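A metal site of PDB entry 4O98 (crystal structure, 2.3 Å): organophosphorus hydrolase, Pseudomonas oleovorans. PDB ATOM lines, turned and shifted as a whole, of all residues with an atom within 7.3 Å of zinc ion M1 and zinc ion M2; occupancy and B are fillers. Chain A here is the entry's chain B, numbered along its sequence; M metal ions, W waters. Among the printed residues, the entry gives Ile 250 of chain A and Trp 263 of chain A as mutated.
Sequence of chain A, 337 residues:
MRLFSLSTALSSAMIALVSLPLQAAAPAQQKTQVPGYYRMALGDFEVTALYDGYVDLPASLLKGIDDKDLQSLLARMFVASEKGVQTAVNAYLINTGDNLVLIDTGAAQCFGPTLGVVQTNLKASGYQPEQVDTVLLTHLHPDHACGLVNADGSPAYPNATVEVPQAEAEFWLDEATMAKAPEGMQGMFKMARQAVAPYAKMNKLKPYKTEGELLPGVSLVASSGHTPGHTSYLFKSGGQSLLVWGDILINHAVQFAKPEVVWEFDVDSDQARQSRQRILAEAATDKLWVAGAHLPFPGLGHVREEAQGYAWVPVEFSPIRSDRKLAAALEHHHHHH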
ATOM      1  N   ALA A  88       0.581 -16.165 -14.160  1.00  0.00           N
ATOM      2  CA  ALA A  88       1.649 -17.117 -13.875  1.00  0.00           C
ATOM      3  C   ALA A  88       2.974 -16.655 -14.483  1.00  0.00           C
ATOM      4  O   ALA A  88       2.984 -15.885 -15.446  1.00  0.00           O
ATOM      5  CB  ALA A  88       1.285 -18.498 -14.407  1.00  0.00           C
ATOM      6  N   VAL A  89       4.074 -17.114 -13.883  1.00  0.00           N
ATOM      7  CA  VAL A  89       5.415 -16.926 -14.430  1.00  0.00           C
ATOM      8  C   VAL A  89       6.060 -18.316 -14.481  1.00  0.00           C
ATOM      9  O   VAL A  89       6.182 -18.980 -13.462  1.00  0.00           O
ATOM     10  CB  VAL A  89       6.272 -15.974 -13.549  1.00  0.00           C
ATOM     11  CG1 VAL A  89       7.734 -15.888 -14.050  1.00  0.00           C
ATOM     12  CG2 VAL A  89       5.637 -14.595 -13.463  1.00  0.00           C
ATOM     13  N   ASP A 104      14.803 -19.554 -19.254  1.00  0.00           N
ATOM     14  CA  ASP A 104      14.315 -18.611 -18.224  1.00  0.00           C
ATOM     15  C   ASP A 104      14.397 -19.218 -16.818  1.00  0.00           C
ATOM     16  O   ASP A 104      14.577 -20.436 -16.660  1.00  0.00           O
ATOM     17  CB  ASP A 104      12.926 -18.050 -18.568  1.00  0.00           C
ATOM     18  CG  ASP A 104      12.941 -17.148 -19.805  1.00  0.00           C
ATOM     19  OD1 ASP A 104      14.057 -16.782 -20.243  1.00  0.00           O
ATOM     20  OD2 ASP A 104      11.860 -16.805 -20.346  1.00  0.00           O
ATOM     21  N   PHE A 111      10.634  -9.645  -7.334  1.00  0.00           N
ATOM     22  CA  PHE A 111       9.278  -9.115  -7.448  1.00  0.00           C
ATOM     23  C   PHE A 111       8.411  -9.467  -6.254  1.00  0.00           C
ATOM     24  O   PHE A 111       7.178  -9.389  -6.328  1.00  0.00           O
ATOM     25  CB  PHE A 111       8.605  -9.593  -8.735  1.00  0.00           C
ATOM     26  CG  PHE A 111       8.922  -8.736  -9.927  1.00  0.00           C
ATOM     27  CD1 PHE A 111       9.605  -7.535  -9.769  1.00  0.00           C
ATOM     28  CD2 PHE A 111       8.513  -9.112 -11.193  1.00  0.00           C
ATOM     29  CE1 PHE A 111       9.897  -6.733 -10.873  1.00  0.00           C
ATOM     30  CE2 PHE A 111       8.798  -8.315 -12.293  1.00  0.00           C
ATOM     31  CZ  PHE A 111       9.481  -7.114 -12.135  1.00  0.00           C
ATOM     32  N   THR A 138      15.113 -15.804 -22.737  1.00  0.00           N
ATOM     33  CA  THR A 138      14.324 -15.199 -23.814  1.00  0.00           C
ATOM     34  C   THR A 138      14.541 -13.681 -23.831  1.00  0.00           C
ATOM     35  O   THR A 138      14.607 -13.070 -24.900  1.00  0.00           O
ATOM     36  CB  THR A 138      12.819 -15.555 -23.705  1.00  0.00           C
ATOM     37  OG1 THR A 138      12.287 -15.088 -22.455  1.00  0.00           O
ATOM     38  CG2 THR A 138      12.628 -17.076 -23.811  1.00  0.00           C
ATOM     39  N   HIS A 139      14.656 -13.090 -22.640  1.00  0.00           N
ATOM     40  CA  HIS A 139      14.989 -11.667 -22.494  1.00  0.00           C
ATOM     41  C   HIS A 139      15.421 -11.392 -21.046  1.00  0.00           C
ATOM     42  O   HIS A 139      15.345 -12.293 -20.208  1.00  0.00           O
ATOM     43  CB  HIS A 139      13.833 -10.748 -22.912  1.00  0.00           C
ATOM     44  CG  HIS A 139      12.560 -10.966 -22.142  1.00  0.00           C
ATOM     45  ND1 HIS A 139      11.970 -12.202 -22.003  1.00  0.00           N
ATOM     46  CD2 HIS A 139      11.734 -10.080 -21.522  1.00  0.00           C
ATOM     47  CE1 HIS A 139      10.847 -12.080 -21.316  1.00  0.00           C
ATOM     48  NE2 HIS A 139      10.674 -10.804 -21.012  1.00  0.00           N
ATOM     49  N   LEU A 140      15.859 -10.169 -20.753  1.00  0.00           N
ATOM     50  CA  LEU A 140      16.453  -9.894 -19.444  1.00  0.00           C
ATOM     51  C   LEU A 140      15.528  -9.256 -18.416  1.00  0.00           C
ATOM     52  O   LEU A 140      15.996  -8.762 -17.387  1.00  0.00           O
ATOM     53  CB  LEU A 140      17.750  -9.075 -19.590  1.00  0.00           C
ATOM     54  CG  LEU A 140      19.027  -9.819 -20.033  1.00  0.00           C
ATOM     55  CD1 LEU A 140      20.136  -8.848 -20.413  1.00  0.00           C
ATOM     56  CD2 LEU A 140      19.537 -10.780 -18.950  1.00  0.00           C
ATOM     57  N   HIS A 141      14.222  -9.272 -18.659  1.00  0.00           N
ATOM     58  CA  HIS A 141      13.282  -8.817 -17.640  1.00  0.00           C
ATOM     59  C   HIS A 141      13.474  -9.584 -16.307  1.00  0.00           C
ATOM     60  O   HIS A 141      13.894 -10.743 -16.311  1.00  0.00           O
ATOM     61  CB  HIS A 141      11.847  -8.967 -18.156  1.00  0.00           C
ATOM     62  CG  HIS A 141      11.304  -7.740 -18.820  1.00  0.00           C
ATOM     63  ND1 HIS A 141      10.107  -7.743 -19.508  1.00  0.00           N
ATOM     64  CD2 HIS A 141      11.779  -6.478 -18.881  1.00  0.00           C
ATOM     65  CE1 HIS A 141       9.869  -6.529 -19.977  1.00  0.00           C
ATOM     66  NE2 HIS A 141      10.869  -5.746 -19.613  1.00  0.00           N
ATOM     67  N   PRO A 142      13.163  -8.946 -15.170  1.00  0.00           N
ATOM     68  CA  PRO A 142      13.515  -9.565 -13.886  1.00  0.00           C
ATOM     69  C   PRO A 142      12.777 -10.885 -13.625  1.00  0.00           C
ATOM     70  O   PRO A 142      13.339 -11.736 -12.925  1.00  0.00           O
ATOM     71  CB  PRO A 142      13.094  -8.515 -12.853  1.00  0.00           C
ATOM     72  CG  PRO A 142      12.883  -7.236 -13.630  1.00  0.00           C
ATOM     73  CD  PRO A 142      12.446  -7.667 -14.990  1.00  0.00           C
ATOM     74  N   ASP A 143      11.556 -11.044 -14.146  1.00  0.00           N
ATOM     75  CA  ASP A 143      10.791 -12.283 -13.962  1.00  0.00           C
ATOM     76  C   ASP A 143      11.329 -13.436 -14.810  1.00  0.00           C
ATOM     77  O   ASP A 143      10.798 -14.555 -14.788  1.00  0.00           O
ATOM     78  CB  ASP A 143       9.287 -12.083 -14.211  1.00  0.00           C
ATOM     79  CG  ASP A 143       8.995 -11.440 -15.557  1.00  0.00           C
ATOM     80  OD1 ASP A 143       9.615 -10.393 -15.850  1.00  0.00           O
ATOM     81  OD2 ASP A 143       8.159 -11.985 -16.316  1.00  0.00           O
ATOM     82  N   HIS A 144      12.397 -13.146 -15.567  1.00  0.00           N
ATOM     83  CA  HIS A 144      13.048 -14.150 -16.391  1.00  0.00           C
ATOM     84  C   HIS A 144      14.530 -14.348 -16.042  1.00  0.00           C
ATOM     85  O   HIS A 144      15.060 -15.460 -16.192  1.00  0.00           O
ATOM     86  CB  HIS A 144      12.888 -13.793 -17.877  1.00  0.00           C
ATOM     87  CG  HIS A 144      11.463 -13.710 -18.315  1.00  0.00           C
ATOM     88  ND1 HIS A 144      10.832 -14.736 -18.986  1.00  0.00           N
ATOM     89  CD2 HIS A 144      10.533 -12.746 -18.124  1.00  0.00           C
ATOM     90  CE1 HIS A 144       9.571 -14.397 -19.201  1.00  0.00           C
ATOM     91  NE2 HIS A 144       9.362 -13.199 -18.690  1.00  0.00           N
ATOM     92  N   HIS A 226       8.891  -6.852 -27.445  1.00  0.00           N
ATOM     93  CA  HIS A 226       8.616  -6.804 -26.009  1.00  0.00           C
ATOM     94  C   HIS A 226       9.843  -6.262 -25.291  1.00  0.00           C
ATOM     95  O   HIS A 226       9.730  -5.486 -24.337  1.00  0.00           O
ATOM     96  CB  HIS A 226       8.247  -8.202 -25.489  1.00  0.00           C
ATOM     97  CG  HIS A 226       8.119  -8.283 -23.993  1.00  0.00           C
ATOM     98  ND1 HIS A 226       7.102  -7.668 -23.296  1.00  0.00           N
ATOM     99  CD2 HIS A 226       8.882  -8.915 -23.074  1.00  0.00           C
ATOM    100  CE1 HIS A 226       7.252  -7.916 -22.008  1.00  0.00           C
ATOM    101  NE2 HIS A 226       8.320  -8.672 -21.847  1.00  0.00           N
ATOM    102  N   THR A 227      11.015  -6.658 -25.783  1.00  0.00           N
ATOM    103  CA  THR A 227      12.280  -6.004 -25.445  1.00  0.00           C
ATOM    104  C   THR A 227      13.091  -6.070 -26.739  1.00  0.00           C
ATOM    105  O   THR A 227      12.703  -6.803 -27.656  1.00  0.00           O
ATOM    106  CB  THR A 227      13.037  -6.715 -24.314  1.00  0.00           C
ATOM    107  OG1 THR A 227      13.376  -8.048 -24.726  1.00  0.00           O
ATOM    108  CG2 THR A 227      12.211  -6.741 -23.028  1.00  0.00           C
ATOM    109  N   HIS A 230      14.443  -9.615 -27.596  1.00  0.00           N
ATOM    110  CA  HIS A 230      13.565 -10.736 -27.207  1.00  0.00           C
ATOM    111  C   HIS A 230      13.637 -11.901 -28.177  1.00  0.00           C
ATOM    112  O   HIS A 230      13.474 -11.754 -29.394  1.00  0.00           O
ATOM    113  CB  HIS A 230      12.115 -10.267 -27.044  1.00  0.00           C
ATOM    114  CG  HIS A 230      11.222 -11.304 -26.433  1.00  0.00           C
ATOM    115  ND1 HIS A 230      10.662 -12.335 -27.159  1.00  0.00           N
ATOM    116  CD2 HIS A 230      10.792 -11.465 -25.153  1.00  0.00           C
ATOM    117  CE1 HIS A 230       9.927 -13.076 -26.360  1.00  0.00           C
ATOM    118  NE2 HIS A 230       9.989 -12.573 -25.138  1.00  0.00           N
ATOM    119  N   GLY A 246       8.795 -17.253 -24.682  1.00  0.00           N
ATOM    120  CA  GLY A 246       9.071 -16.083 -23.865  1.00  0.00           C
ATOM    121  C   GLY A 246       7.800 -15.302 -23.588  1.00  0.00           C
ATOM    122  O   GLY A 246       6.782 -15.882 -23.190  1.00  0.00           O
ATOM    123  N   ASP A 247       7.855 -13.986 -23.826  1.00  0.00           N
ATOM    124  CA  ASP A 247       6.723 -13.122 -23.572  1.00  0.00           C
ATOM    125  C   ASP A 247       6.108 -12.550 -24.874  1.00  0.00           C
ATOM    126  O   ASP A 247       5.732 -11.392 -24.921  1.00  0.00           O
ATOM    127  CB  ASP A 247       7.123 -11.968 -22.622  1.00  0.00           C
ATOM    128  CG  ASP A 247       7.418 -12.435 -21.188  1.00  0.00           C
ATOM    129  OD1 ASP A 247       7.429 -13.656 -20.942  1.00  0.00           O
ATOM    130  OD2 ASP A 247       7.647 -11.567 -20.321  1.00  0.00           O
ATOM    131  N   LEU A 249       3.374 -12.893 -25.701  1.00  0.00           N
ATOM    132  CA  LEU A 249       1.991 -12.713 -25.298  1.00  0.00           C
ATOM    133  C   LEU A 249       1.934 -12.835 -23.768  1.00  0.00           C
ATOM    134  O   LEU A 249       2.581 -13.722 -23.201  1.00  0.00           O
ATOM    135  CB  LEU A 249       1.189 -13.825 -25.960  1.00  0.00           C
ATOM    136  CG  LEU A 249      -0.299 -13.909 -25.929  1.00  0.00           C
ATOM    137  CD1 LEU A 249      -0.727 -14.672 -27.162  1.00  0.00           C
ATOM    138  CD2 LEU A 249      -0.757 -14.618 -24.665  1.00  0.00           C
ATOM    139  N   ILE A 250       1.170 -11.955 -23.105  1.00  0.00           N
ATOM    140  CA  ILE A 250       1.093 -11.909 -21.641  1.00  0.00           C
ATOM    141  C   ILE A 250      -0.259 -12.375 -21.070  1.00  0.00           C
ATOM    142  O   ILE A 250      -0.335 -12.879 -19.940  1.00  0.00           O
ATOM    143  CB  ILE A 250       1.368 -10.485 -21.119  1.00  0.00           C
ATOM    144  CG1 ILE A 250       2.636  -9.903 -21.747  1.00  0.00           C
ATOM    145  CG2 ILE A 250       1.460 -10.474 -19.599  1.00  0.00           C
ATOM    146  CD1 ILE A 250       3.904 -10.613 -21.327  1.00  0.00           C
ATOM    147  N   TRP A 263       0.804  -4.540 -24.813  1.00  0.00           N
ATOM    148  CA  TRP A 263       1.093  -4.557 -23.396  1.00  0.00           C
ATOM    149  C   TRP A 263       1.904  -3.305 -23.044  1.00  0.00           C
ATOM    150  O   TRP A 263       2.814  -2.934 -23.789  1.00  0.00           O
ATOM    151  CB  TRP A 263       1.875  -5.844 -23.090  1.00  0.00           C
ATOM    152  CG  TRP A 263       2.310  -6.042 -21.670  1.00  0.00           C
ATOM    153  CD1 TRP A 263       3.582  -5.993 -21.185  1.00  0.00           C
ATOM    154  CD2 TRP A 263       1.465  -6.365 -20.555  1.00  0.00           C
ATOM    155  NE1 TRP A 263       3.588  -6.242 -19.837  1.00  0.00           N
ATOM    156  CE2 TRP A 263       2.301  -6.478 -19.424  1.00  0.00           C
ATOM    157  CE3 TRP A 263       0.090  -6.569 -20.406  1.00  0.00           C
ATOM    158  CZ2 TRP A 263       1.798  -6.779 -18.156  1.00  0.00           C
ATOM    159  CZ3 TRP A 263      -0.401  -6.866 -19.163  1.00  0.00           C
ATOM    160  CH2 TRP A 263       0.446  -6.974 -18.058  1.00  0.00           C
ATOM    161  N   PHE A 265       4.243  -2.709 -21.101  1.00  0.00           N
ATOM    162  CA  PHE A 265       5.677  -2.879 -20.871  1.00  0.00           C
ATOM    163  C   PHE A 265       6.417  -3.451 -22.059  1.00  0.00           C
ATOM    164  O   PHE A 265       7.608  -3.778 -21.953  1.00  0.00           O
ATOM    165  CB  PHE A 265       5.929  -3.734 -19.636  1.00  0.00           C
ATOM    166  CG  PHE A 265       5.483  -3.090 -18.379  1.00  0.00           C
ATOM    167  CD1 PHE A 265       6.230  -2.056 -17.819  1.00  0.00           C
ATOM    168  CD2 PHE A 265       4.329  -3.500 -17.746  1.00  0.00           C
ATOM    169  CE1 PHE A 265       5.818  -1.453 -16.639  1.00  0.00           C
ATOM    170  CE2 PHE A 265       3.917  -2.897 -16.567  1.00  0.00           C
ATOM    171  CZ  PHE A 265       4.660  -1.870 -16.025  1.00  0.00           C
ATOM    172  N   ASP A 266       5.725  -3.586 -23.183  1.00  0.00           N
ATOM    173  CA  ASP A 266       6.415  -3.872 -24.430  1.00  0.00           C
ATOM    174  C   ASP A 266       7.295  -2.641 -24.665  1.00  0.00           C
ATOM    175  O   ASP A 266       6.787  -1.519 -24.685  1.00  0.00           O
ATOM    176  CB  ASP A 266       5.405  -4.047 -25.567  1.00  0.00           C
ATOM    177  CG  ASP A 266       4.664  -5.384 -25.515  1.00  0.00           C
ATOM    178  OD1 ASP A 266       5.192  -6.353 -24.939  1.00  0.00           O
ATOM    179  OD2 ASP A 266       3.546  -5.454 -26.076  1.00  0.00           O
ATOM    180  N   ALA A 293       5.831 -18.375 -21.193  1.00  0.00           N
ATOM    181  CA  ALA A 293       6.207 -17.895 -19.861  1.00  0.00           C
ATOM    182  C   ALA A 293       5.064 -17.352 -19.006  1.00  0.00           C
ATOM    183  O   ALA A 293       5.108 -17.478 -17.785  1.00  0.00           O
ATOM    184  CB  ALA A 293       7.299 -16.835 -19.989  1.00  0.00           C
ATOM    185  N   HIS A 294       4.058 -16.729 -19.629  1.00  0.00           N
ATOM    186  CA  HIS A 294       2.932 -16.186 -18.853  1.00  0.00           C
ATOM    187  C   HIS A 294       1.558 -16.813 -19.126  1.00  0.00           C
ATOM    188  O   HIS A 294       0.523 -16.284 -18.728  1.00  0.00           O
ATOM    189  CB  HIS A 294       2.861 -14.664 -18.978  1.00  0.00           C
ATOM    190  CG  HIS A 294       4.092 -13.974 -18.453  1.00  0.00           C
ATOM    191  ND1 HIS A 294       4.483 -14.087 -17.141  1.00  0.00           N
ATOM    192  CD2 HIS A 294       5.020 -13.222 -19.066  1.00  0.00           C
ATOM    193  CE1 HIS A 294       5.607 -13.411 -16.967  1.00  0.00           C
ATOM    194  NE2 HIS A 294       5.947 -12.867 -18.118  1.00  0.00           N
HETATM  195 ZN    ZN M   1       7.754 -11.935 -18.412  1.00  0.00          ZN
HETATM  196 ZN    ZN M   2       8.935  -9.604 -20.126  1.00  0.00          ZN
HETATM  197  O   HOH W   1       8.367  -9.861 -18.107  1.00  0.00           O
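Zinc ion M1 is bound by OD2 of Asp 247, NE2 of His 294, NE2 of His 144, OD2 of Asp 143 and water W1. Zinc ion M1 has five donor atoms within binding distance.
N of Asp 247 is in hydrogen-bond range of NE2 of His 230, 2.9 Å away. A ring nitrogen (ND1) of His 226 sits at hydrogen-bond distance from the side-chain carboxylate of Asp 266 (2.8 Å). A ring nitrogen (ND1) of His 294 lies within hydrogen-bond range of the backbone carbonyl oxygen (O) of Ala 88 (2.9 Å). The side-chain carboxylate (OD2) of Asp 104 sits at hydrogen-bond distance from a ring nitrogen (ND1) of His 144, 2.7 Å away. OG1 of Thr 138 sits at hydrogen-bond distance from ND1 of His 139, at 2.9 Å.
Of the 23 residues printed, 5 come within 4 Å of zinc ion M2. Along chain A the residues within 4 Å of zinc ion M2 span positions 139 to 247.
NE2 of His 226 binds zinc ion M2 (2.1 Å). Water W1 is bound to zinc ion M2. ND1 of His 141 binds zinc ion M2 (2.3 Å). NE2 of His 139 is bound to zinc ion M2. Zinc ion M2 is bound by the side-chain carboxylate (OD2) of Asp 247.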
